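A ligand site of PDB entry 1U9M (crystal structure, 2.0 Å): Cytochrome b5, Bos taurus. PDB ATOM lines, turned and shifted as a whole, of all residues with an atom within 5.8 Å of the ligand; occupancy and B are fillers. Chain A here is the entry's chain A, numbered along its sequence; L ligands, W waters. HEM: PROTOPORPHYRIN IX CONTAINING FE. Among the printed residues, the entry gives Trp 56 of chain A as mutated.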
ATOM      1  N   LEU A  21     -17.005 -15.931  33.451  1.00  0.00           N
ATOM      2  CA  LEU A  21     -15.970 -15.462  34.349  1.00  0.00           C
ATOM      3  C   LEU A  21     -16.036 -13.945  34.479  1.00  0.00           C
ATOM      4  O   LEU A  21     -16.664 -13.253  33.669  1.00  0.00           O
ATOM      5  CB  LEU A  21     -14.571 -15.921  33.891  1.00  0.00           C
ATOM      6  CG  LEU A  21     -13.995 -15.571  32.522  1.00  0.00           C
ATOM      7  CD1 LEU A  21     -13.659 -14.086  32.441  1.00  0.00           C
ATOM      8  CD2 LEU A  21     -12.731 -16.399  32.338  1.00  0.00           C
ATOM      9  N   LEU A  23     -14.182 -10.179  34.941  1.00  0.00           N
ATOM     10  CA  LEU A  23     -13.029  -9.332  34.646  1.00  0.00           C
ATOM     11  C   LEU A  23     -13.469  -7.957  35.153  1.00  0.00           C
ATOM     12  O   LEU A  23     -14.391  -7.345  34.598  1.00  0.00           O
ATOM     13  CB  LEU A  23     -12.708  -9.279  33.147  1.00  0.00           C
ATOM     14  CG  LEU A  23     -12.327 -10.600  32.491  1.00  0.00           C
ATOM     15  CD1 LEU A  23     -11.909 -10.354  31.042  1.00  0.00           C
ATOM     16  CD2 LEU A  23     -11.173 -11.246  33.264  1.00  0.00           C
ATOM     17  N   TYR A  28     -18.352 -12.199  31.596  1.00  0.00           N
ATOM     18  CA  TYR A  28     -18.092 -12.649  30.239  1.00  0.00           C
ATOM     19  C   TYR A  28     -18.482 -14.107  30.015  1.00  0.00           C
ATOM     20  O   TYR A  28     -18.239 -14.961  30.866  1.00  0.00           O
ATOM     21  CB  TYR A  28     -16.596 -12.509  29.894  1.00  0.00           C
ATOM     22  CG  TYR A  28     -16.052 -11.093  30.033  1.00  0.00           C
ATOM     23  CD1 TYR A  28     -16.009 -10.458  31.277  1.00  0.00           C
ATOM     24  CD2 TYR A  28     -15.595 -10.394  28.911  1.00  0.00           C
ATOM     25  CE1 TYR A  28     -15.523  -9.152  31.394  1.00  0.00           C
ATOM     26  CE2 TYR A  28     -15.116  -9.095  29.025  1.00  0.00           C
ATOM     27  CZ  TYR A  28     -15.080  -8.481  30.266  1.00  0.00           C
ATOM     28  OH  TYR A  28     -14.594  -7.204  30.381  1.00  0.00           O
ATOM     29  N   LEU A  30     -17.560 -16.951  27.697  1.00  0.00           N
ATOM     30  CA  LEU A  30     -16.550 -17.382  26.737  1.00  0.00           C
ATOM     31  C   LEU A  30     -16.796 -18.746  26.112  1.00  0.00           C
ATOM     32  O   LEU A  30     -15.948 -19.275  25.403  1.00  0.00           O
ATOM     33  CB  LEU A  30     -15.170 -17.382  27.402  1.00  0.00           C
ATOM     34  CG  LEU A  30     -14.750 -16.076  28.104  1.00  0.00           C
ATOM     35  CD1 LEU A  30     -13.348 -16.249  28.692  1.00  0.00           C
ATOM     36  CD2 LEU A  30     -14.775 -14.914  27.124  1.00  0.00           C
ATOM     37  N   PHE A  33     -15.900 -19.181  22.719  1.00  0.00           N
ATOM     38  CA  PHE A  33     -14.570 -18.653  22.475  1.00  0.00           C
ATOM     39  C   PHE A  33     -13.472 -19.617  22.923  1.00  0.00           C
ATOM     40  O   PHE A  33     -12.312 -19.492  22.515  1.00  0.00           O
ATOM     41  CB  PHE A  33     -14.404 -17.315  23.201  1.00  0.00           C
ATOM     42  CG  PHE A  33     -13.096 -16.636  22.928  1.00  0.00           C
ATOM     43  CD1 PHE A  33     -12.150 -16.483  23.939  1.00  0.00           C
ATOM     44  CD2 PHE A  33     -12.800 -16.137  21.667  1.00  0.00           C
ATOM     45  CE1 PHE A  33     -10.940 -15.846  23.699  1.00  0.00           C
ATOM     46  CE2 PHE A  33     -11.592 -15.505  21.405  1.00  0.00           C
ATOM     47  CZ  PHE A  33     -10.655 -15.360  22.423  1.00  0.00           C
ATOM     48  N   HIS A  37      -9.596 -19.394  21.468  1.00  0.00           N
ATOM     49  CA  HIS A  37      -8.619 -18.669  22.270  1.00  0.00           C
ATOM     50  C   HIS A  37      -7.169 -19.017  21.937  1.00  0.00           C
ATOM     51  O   HIS A  37      -6.736 -20.140  22.138  1.00  0.00           O
ATOM     52  CB  HIS A  37      -8.878 -18.970  23.751  1.00  0.00           C
ATOM     53  CG  HIS A  37      -8.038 -18.166  24.686  1.00  0.00           C
ATOM     54  ND1 HIS A  37      -7.559 -18.644  25.883  1.00  0.00           N
ATOM     55  CD2 HIS A  37      -7.641 -16.867  24.621  1.00  0.00           C
ATOM     56  CE1 HIS A  37      -6.901 -17.659  26.497  1.00  0.00           C
ATOM     57  NE2 HIS A  37      -6.923 -16.555  25.764  1.00  0.00           N
ATOM     58  N   PRO A  38      -6.394 -18.034  21.439  1.00  0.00           N
ATOM     59  CA  PRO A  38      -4.990 -18.302  21.098  1.00  0.00           C
ATOM     60  C   PRO A  38      -4.222 -18.859  22.298  1.00  0.00           C
ATOM     61  O   PRO A  38      -3.256 -19.596  22.141  1.00  0.00           O
ATOM     62  CB  PRO A  38      -4.481 -16.933  20.663  1.00  0.00           C
ATOM     63  CG  PRO A  38      -5.688 -16.304  20.051  1.00  0.00           C
ATOM     64  CD  PRO A  38      -6.776 -16.673  21.037  1.00  0.00           C
ATOM     65  N   GLY A  39      -4.662 -18.493  23.496  1.00  0.00           N
ATOM     66  CA  GLY A  39      -3.995 -18.977  24.704  1.00  0.00           C
ATOM     67  C   GLY A  39      -4.435 -20.373  25.095  1.00  0.00           C
ATOM     68  O   GLY A  39      -4.013 -20.896  26.118  1.00  0.00           O
ATOM     69  N   VAL A  43      -6.407 -23.029  29.914  1.00  0.00           N
ATOM     70  CA  VAL A  43      -6.183 -21.917  30.819  1.00  0.00           C
ATOM     71  C   VAL A  43      -7.510 -21.270  31.204  1.00  0.00           C
ATOM     72  O   VAL A  43      -7.710 -20.863  32.336  1.00  0.00           O
ATOM     73  CB  VAL A  43      -5.242 -20.859  30.206  1.00  0.00           C
ATOM     74  CG1 VAL A  43      -5.900 -20.199  29.021  1.00  0.00           C
ATOM     75  CG2 VAL A  43      -4.856 -19.830  31.256  1.00  0.00           C
ATOM     76  N   LEU A  44      -8.429 -21.199  30.235  1.00  0.00           N
ATOM     77  CA  LEU A  44      -9.736 -20.601  30.488  1.00  0.00           C
ATOM     78  C   LEU A  44     -10.620 -21.472  31.377  1.00  0.00           C
ATOM     79  O   LEU A  44     -11.328 -20.950  32.239  1.00  0.00           O
ATOM     80  CB  LEU A  44     -10.452 -20.335  29.160  1.00  0.00           C
ATOM     81  CG  LEU A  44      -9.783 -19.308  28.251  1.00  0.00           C
ATOM     82  CD1 LEU A  44     -10.506 -19.226  26.921  1.00  0.00           C
ATOM     83  CD2 LEU A  44      -9.779 -17.957  28.954  1.00  0.00           C
ATOM     84  N   GLN A  47     -10.042 -21.037  35.066  1.00  0.00           N
ATOM     85  CA  GLN A  47     -10.555 -19.798  35.629  1.00  0.00           C
ATOM     86  C   GLN A  47     -12.073 -19.680  35.587  1.00  0.00           C
ATOM     87  O   GLN A  47     -12.652 -18.813  36.224  1.00  0.00           O
ATOM     88  CB  GLN A  47      -9.927 -18.612  34.894  1.00  0.00           C
ATOM     89  CG  GLN A  47      -8.432 -18.497  35.057  1.00  0.00           C
ATOM     90  CD  GLN A  47      -8.023 -18.295  36.503  1.00  0.00           C
ATOM     91  OE1 GLN A  47      -8.574 -17.433  37.199  1.00  0.00           O
ATOM     92  NE2 GLN A  47      -7.063 -19.079  36.975  1.00  0.00           N
ATOM     93  N   ALA A  52     -11.262 -13.725  37.246  1.00  0.00           N
ATOM     94  CA  ALA A  52      -9.968 -13.986  36.614  1.00  0.00           C
ATOM     95  C   ALA A  52      -9.179 -12.724  36.292  1.00  0.00           C
ATOM     96  O   ALA A  52      -8.206 -12.779  35.552  1.00  0.00           O
ATOM     97  CB  ALA A  52     -10.185 -14.785  35.333  1.00  0.00           C
ATOM     98  N   ASN A  55      -5.240 -12.867  36.653  1.00  0.00           N
ATOM     99  CA  ASN A  55      -4.619 -13.763  35.673  1.00  0.00           C
ATOM    100  C   ASN A  55      -4.661 -13.114  34.305  1.00  0.00           C
ATOM    101  O   ASN A  55      -3.692 -13.160  33.553  1.00  0.00           O
ATOM    102  CB  ASN A  55      -5.377 -15.095  35.635  1.00  0.00           C
ATOM    103  CG  ASN A  55      -5.512 -15.739  37.006  1.00  0.00           C
ATOM    104  OD1 ASN A  55      -4.565 -16.335  37.526  1.00  0.00           O
ATOM    105  ND2 ASN A  55      -6.679 -15.600  37.614  1.00  0.00           N
ATOM    106  N   TRP A  56      -5.797 -12.498  33.993  1.00  0.00           N
ATOM    107  CA  TRP A  56      -5.996 -11.823  32.718  1.00  0.00           C
ATOM    108  C   TRP A  56      -5.006 -10.680  32.529  1.00  0.00           C
ATOM    109  O   TRP A  56      -4.460 -10.490  31.455  1.00  0.00           O
ATOM    110  CB  TRP A  56      -7.460 -11.326  32.620  1.00  0.00           C
ATOM    111  CG  TRP A  56      -7.678 -10.096  31.767  1.00  0.00           C
ATOM    112  CD1 TRP A  56      -7.714  -8.805  32.205  1.00  0.00           C
ATOM    113  CD2 TRP A  56      -7.880 -10.050  30.351  1.00  0.00           C
ATOM    114  NE1 TRP A  56      -7.931  -7.952  31.154  1.00  0.00           N
ATOM    115  CE2 TRP A  56      -8.034  -8.691  30.002  1.00  0.00           C
ATOM    116  CE3 TRP A  56      -7.938 -11.018  29.344  1.00  0.00           C
ATOM    117  CZ2 TRP A  56      -8.239  -8.275  28.679  1.00  0.00           C
ATOM    118  CZ3 TRP A  56      -8.145 -10.603  28.031  1.00  0.00           C
ATOM    119  CH2 TRP A  56      -8.300  -9.239  27.713  1.00  0.00           C
ATOM    120  N   VAL A  59      -0.736 -12.011  32.384  1.00  0.00           N
ATOM    121  CA  VAL A  59      -0.201 -12.620  31.177  1.00  0.00           C
ATOM    122  C   VAL A  59       0.119 -11.655  30.033  1.00  0.00           C
ATOM    123  O   VAL A  59       0.657 -12.063  29.005  1.00  0.00           O
ATOM    124  CB  VAL A  59      -1.124 -13.733  30.649  1.00  0.00           C
ATOM    125  CG1 VAL A  59      -1.180 -14.867  31.660  1.00  0.00           C
ATOM    126  CG2 VAL A  59      -2.512 -13.199  30.387  1.00  0.00           C
ATOM    127  N   GLY A  60      -0.213 -10.382  30.211  1.00  0.00           N
ATOM    128  CA  GLY A  60       0.074  -9.381  29.194  1.00  0.00           C
ATOM    129  C   GLY A  60      -0.699  -9.462  27.883  1.00  0.00           C
ATOM    130  O   GLY A  60      -0.112  -9.656  26.819  1.00  0.00           O
ATOM    131  N   HIS A  61      -2.024  -9.312  27.949  1.00  0.00           N
ATOM    132  CA  HIS A  61      -2.839  -9.356  26.742  1.00  0.00           C
ATOM    133  C   HIS A  61      -2.625  -8.102  25.896  1.00  0.00           C
ATOM    134  O   HIS A  61      -2.402  -7.022  26.426  1.00  0.00           O
ATOM    135  CB  HIS A  61      -4.323  -9.469  27.102  1.00  0.00           C
ATOM    136  CG  HIS A  61      -4.746 -10.862  27.435  1.00  0.00           C
ATOM    137  ND1 HIS A  61      -4.699 -11.419  28.694  1.00  0.00           N
ATOM    138  CD2 HIS A  61      -5.208 -11.847  26.615  1.00  0.00           C
ATOM    139  CE1 HIS A  61      -5.100 -12.686  28.593  1.00  0.00           C
ATOM    140  NE2 HIS A  61      -5.424 -12.988  27.353  1.00  0.00           N
ATOM    141  N   SER A  62      -2.707  -8.256  24.575  1.00  0.00           N
ATOM    142  CA  SER A  62      -2.511  -7.139  23.665  1.00  0.00           C
ATOM    143  C   SER A  62      -3.743  -6.233  23.613  1.00  0.00           C
ATOM    144  O   SER A  62      -4.826  -6.610  24.049  1.00  0.00           O
ATOM    145  CB  SER A  62      -2.240  -7.658  22.255  1.00  0.00           C
ATOM    146  OG  SER A  62      -3.438  -8.121  21.656  1.00  0.00           O
ATOM    147  N   ASP A  64      -5.289  -5.544  21.101  1.00  0.00           N
ATOM    148  CA  ASP A  64      -6.218  -6.229  20.211  1.00  0.00           C
ATOM    149  C   ASP A  64      -7.072  -7.195  21.030  1.00  0.00           C
ATOM    150  O   ASP A  64      -8.285  -7.261  20.865  1.00  0.00           O
ATOM    151  CB  ASP A  64      -5.474  -7.007  19.125  1.00  0.00           C
ATOM    152  CG  ASP A  64      -4.894  -6.108  18.039  1.00  0.00           C
ATOM    153  OD1 ASP A  64      -4.046  -6.597  17.259  1.00  0.00           O
ATOM    154  OD2 ASP A  64      -5.276  -4.917  17.959  1.00  0.00           O
ATOM    155  N   ALA A  65      -6.417  -7.942  21.918  1.00  0.00           N
ATOM    156  CA  ALA A  65      -7.121  -8.907  22.748  1.00  0.00           C
ATOM    157  C   ALA A  65      -8.128  -8.196  23.662  1.00  0.00           C
ATOM    158  O   ALA A  65      -9.218  -8.723  23.911  1.00  0.00           O
ATOM    159  CB  ALA A  65      -6.127  -9.700  23.572  1.00  0.00           C
ATOM    160  N   LEU A  68     -11.302  -7.222  21.774  1.00  0.00           N
ATOM    161  CA  LEU A  68     -12.065  -8.423  21.451  1.00  0.00           C
ATOM    162  C   LEU A  68     -12.810  -8.985  22.656  1.00  0.00           C
ATOM    163  O   LEU A  68     -13.860  -9.622  22.504  1.00  0.00           O
ATOM    164  CB  LEU A  68     -11.141  -9.508  20.887  1.00  0.00           C
ATOM    165  CG  LEU A  68     -11.767 -10.881  20.655  1.00  0.00           C
ATOM    166  CD1 LEU A  68     -12.959 -10.763  19.727  1.00  0.00           C
ATOM    167  CD2 LEU A  68     -10.735 -11.833  20.066  1.00  0.00           C
ATOM    168  N   SER A  69     -12.280  -8.763  23.856  1.00  0.00           N
ATOM    169  CA  SER A  69     -12.935  -9.285  25.058  1.00  0.00           C
ATOM    170  C   SER A  69     -14.333  -8.707  25.211  1.00  0.00           C
ATOM    171  O   SER A  69     -15.267  -9.398  25.639  1.00  0.00           O
ATOM    172  CB  SER A  69     -12.106  -8.960  26.305  1.00  0.00           C
ATOM    173  OG  SER A  69     -12.107  -7.566  26.551  1.00  0.00           O
ATOM    174  N   PHE A  72     -17.754 -10.344  24.342  1.00  0.00           N
ATOM    175  CA  PHE A  72     -18.283 -11.458  25.129  1.00  0.00           C
ATOM    176  C   PHE A  72     -19.019 -11.055  26.423  1.00  0.00           C
ATOM    177  O   PHE A  72     -19.437 -11.910  27.193  1.00  0.00           O
ATOM    178  CB  PHE A  72     -17.144 -12.417  25.484  1.00  0.00           C
ATOM    179  CG  PHE A  72     -16.469 -13.009  24.276  1.00  0.00           C
ATOM    180  CD1 PHE A  72     -17.108 -13.978  23.513  1.00  0.00           C
ATOM    181  CD2 PHE A  72     -15.211 -12.575  23.882  1.00  0.00           C
ATOM    182  CE1 PHE A  72     -16.498 -14.508  22.363  1.00  0.00           C
ATOM    183  CE2 PHE A  72     -14.590 -13.092  22.747  1.00  0.00           C
ATOM    184  CZ  PHE A  72     -15.242 -14.061  21.979  1.00  0.00           C
HETATM  185  CHA HEM L   1      -3.298 -15.045  24.677  1.00  0.00           C
HETATM  186  CHB HEM L   1      -7.674 -13.125  23.859  1.00  0.00           C
HETATM  187  CHC HEM L   1      -8.950 -14.340  28.373  1.00  0.00           C
HETATM  188  CHD HEM L   1      -4.660 -16.389  29.138  1.00  0.00           C
HETATM  189  C1A HEM L   1      -4.376 -14.391  24.081  1.00  0.00           C
HETATM  190  C2A HEM L   1      -4.375 -13.794  22.733  1.00  0.00           C
HETATM  191  C3A HEM L   1      -5.590 -13.274  22.508  1.00  0.00           C
HETATM  192  C4A HEM L   1      -6.368 -13.543  23.690  1.00  0.00           C
HETATM  193  CMA HEM L   1      -6.033 -12.516  21.253  1.00  0.00           C
HETATM  194  CAA HEM L   1      -3.182 -13.664  21.784  1.00  0.00           C
HETATM  195  CBA HEM L   1      -2.113 -12.718  22.312  1.00  0.00           C
HETATM  196  CGA HEM L   1      -2.634 -11.323  22.528  1.00  0.00           C
HETATM  197  O1A HEM L   1      -3.147 -10.723  21.556  1.00  0.00           O
HETATM  198  O2A HEM L   1      -2.523 -10.811  23.669  1.00  0.00           O
HETATM  199  C1B HEM L   1      -8.411 -13.317  25.036  1.00  0.00           C
HETATM  200  C2B HEM L   1      -9.785 -12.917  25.207  1.00  0.00           C
HETATM  201  C3B HEM L   1     -10.146 -13.286  26.458  1.00  0.00           C
HETATM  202  C4B HEM L   1      -8.978 -13.894  27.081  1.00  0.00           C
HETATM  203  CMB HEM L   1     -10.715 -12.221  24.219  1.00  0.00           C
HETATM  204  CAB HEM L   1     -11.446 -13.258  26.971  1.00  0.00           C
HETATM  205  CBB HEM L   1     -11.940 -12.156  27.655  1.00  0.00           C
HETATM  206  C1C HEM L   1      -7.880 -14.944  28.979  1.00  0.00           C
HETATM  207  C2C HEM L   1      -7.873 -15.318  30.384  1.00  0.00           C
HETATM  208  C3C HEM L   1      -6.664 -15.915  30.593  1.00  0.00           C
HETATM  209  C4C HEM L   1      -5.961 -15.908  29.323  1.00  0.00           C
HETATM  210  CMC HEM L   1      -8.955 -14.925  31.415  1.00  0.00           C
HETATM  211  CAC HEM L   1      -6.066 -16.298  31.798  1.00  0.00           C
HETATM  212  CBC HEM L   1      -6.702 -16.849  32.899  1.00  0.00           C
HETATM  213  C1D HEM L   1      -3.948 -16.260  27.961  1.00  0.00           C
HETATM  214  C2D HEM L   1      -2.621 -16.805  27.748  1.00  0.00           C
HETATM  215  C3D HEM L   1      -2.251 -16.471  26.488  1.00  0.00           C
HETATM  216  C4D HEM L   1      -3.319 -15.650  25.936  1.00  0.00           C
HETATM  217  CMD HEM L   1      -1.768 -17.523  28.776  1.00  0.00           C
HETATM  218  CAD HEM L   1      -1.009 -16.987  25.764  1.00  0.00           C
HETATM  219  CBD HEM L   1       0.154 -16.015  25.853  1.00  0.00           C
HETATM  220  CGD HEM L   1       1.437 -16.591  25.262  1.00  0.00           C
HETATM  221  O1D HEM L   1       2.497 -15.946  25.407  1.00  0.00           O
HETATM  222  O2D HEM L   1       1.396 -17.685  24.658  1.00  0.00           O
HETATM  223  NA  HEM L   1      -5.608 -14.221  24.663  1.00  0.00           N
HETATM  224  NB  HEM L   1      -7.904 -13.914  26.193  1.00  0.00           N
HETATM  225  NC  HEM L   1      -6.696 -15.266  28.334  1.00  0.00           N
HETATM  226  ND  HEM L   1      -4.396 -15.580  26.815  1.00  0.00           N
HETATM  227 FE   HEM L   1      -6.152 -14.750  26.498  1.00  0.00          FE
HETATM  228  O   HOH W   1      -2.590 -10.904  19.082  1.00  0.00           O
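The backbone NH (N) of Ser 62 sits at hydrogen-bond distance from an oxygen (O2A) of the ligand (2.7 Å). A ring nitrogen (NE2) of His 61 is bound to an iron atom (FE) of the ligand (2.1 Å). The side-chain hydroxyl (OG) of Ser 62 is in hydrogen-bond range of an oxygen (O1A) of the ligand (2.6 Å). A ring nitrogen (NE2) of His 37 binds an iron atom (FE) of the ligand, 2.1 Å away.
The backbone carbonyl oxygen of Trp 56 sits at hydrogen-bond distance from a ring nitrogen (ND1) of His 61 (2.9 Å). The side-chain amide nitrogen (ND2) of Asn 55 is in hydrogen-bond range of the side-chain amide oxygen (OE1) of Gln 47, at 2.7 Å. The side-chain hydroxyl (OG) of Ser 62 sits close to the backbone NH (N) of Asp 64 (3.2 Å). N of Ala 65 is in hydrogen-bond range of OG of Ser 62, at 3.0 Å.
CD1 of Leu 23 touches CBB of the ligand, at 3.8 Å. Leu 30 touches the ligand. Phe 33 touches the ligand (CE1 to C2B, 3.5 Å). Pro 38 touches the ligand (CB to CAA, 3.7 Å). Gly 39 touches the ligand. Val 43 touches the ligand. CD2 of Leu 44 touches C2C of the ligand, 3.6 Å away. Gln 47 touches the ligand. Asn 55 touches the ligand. Trp 56 touches the ligand (CZ3 to C4B, 3.5 Å). Val 59 touches the ligand. Ala 65 touches the ligand (CB to CMA, 3.6 Å). CG of Leu 68 touches CMB of the ligand (3.95 Å). Ser 69 touches the ligand. Of the 23 residues printed, 17 come within 4 Å of the ligand. The nearest printed residue that does not touch the ligand is Ala 52 (4.1 Å).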
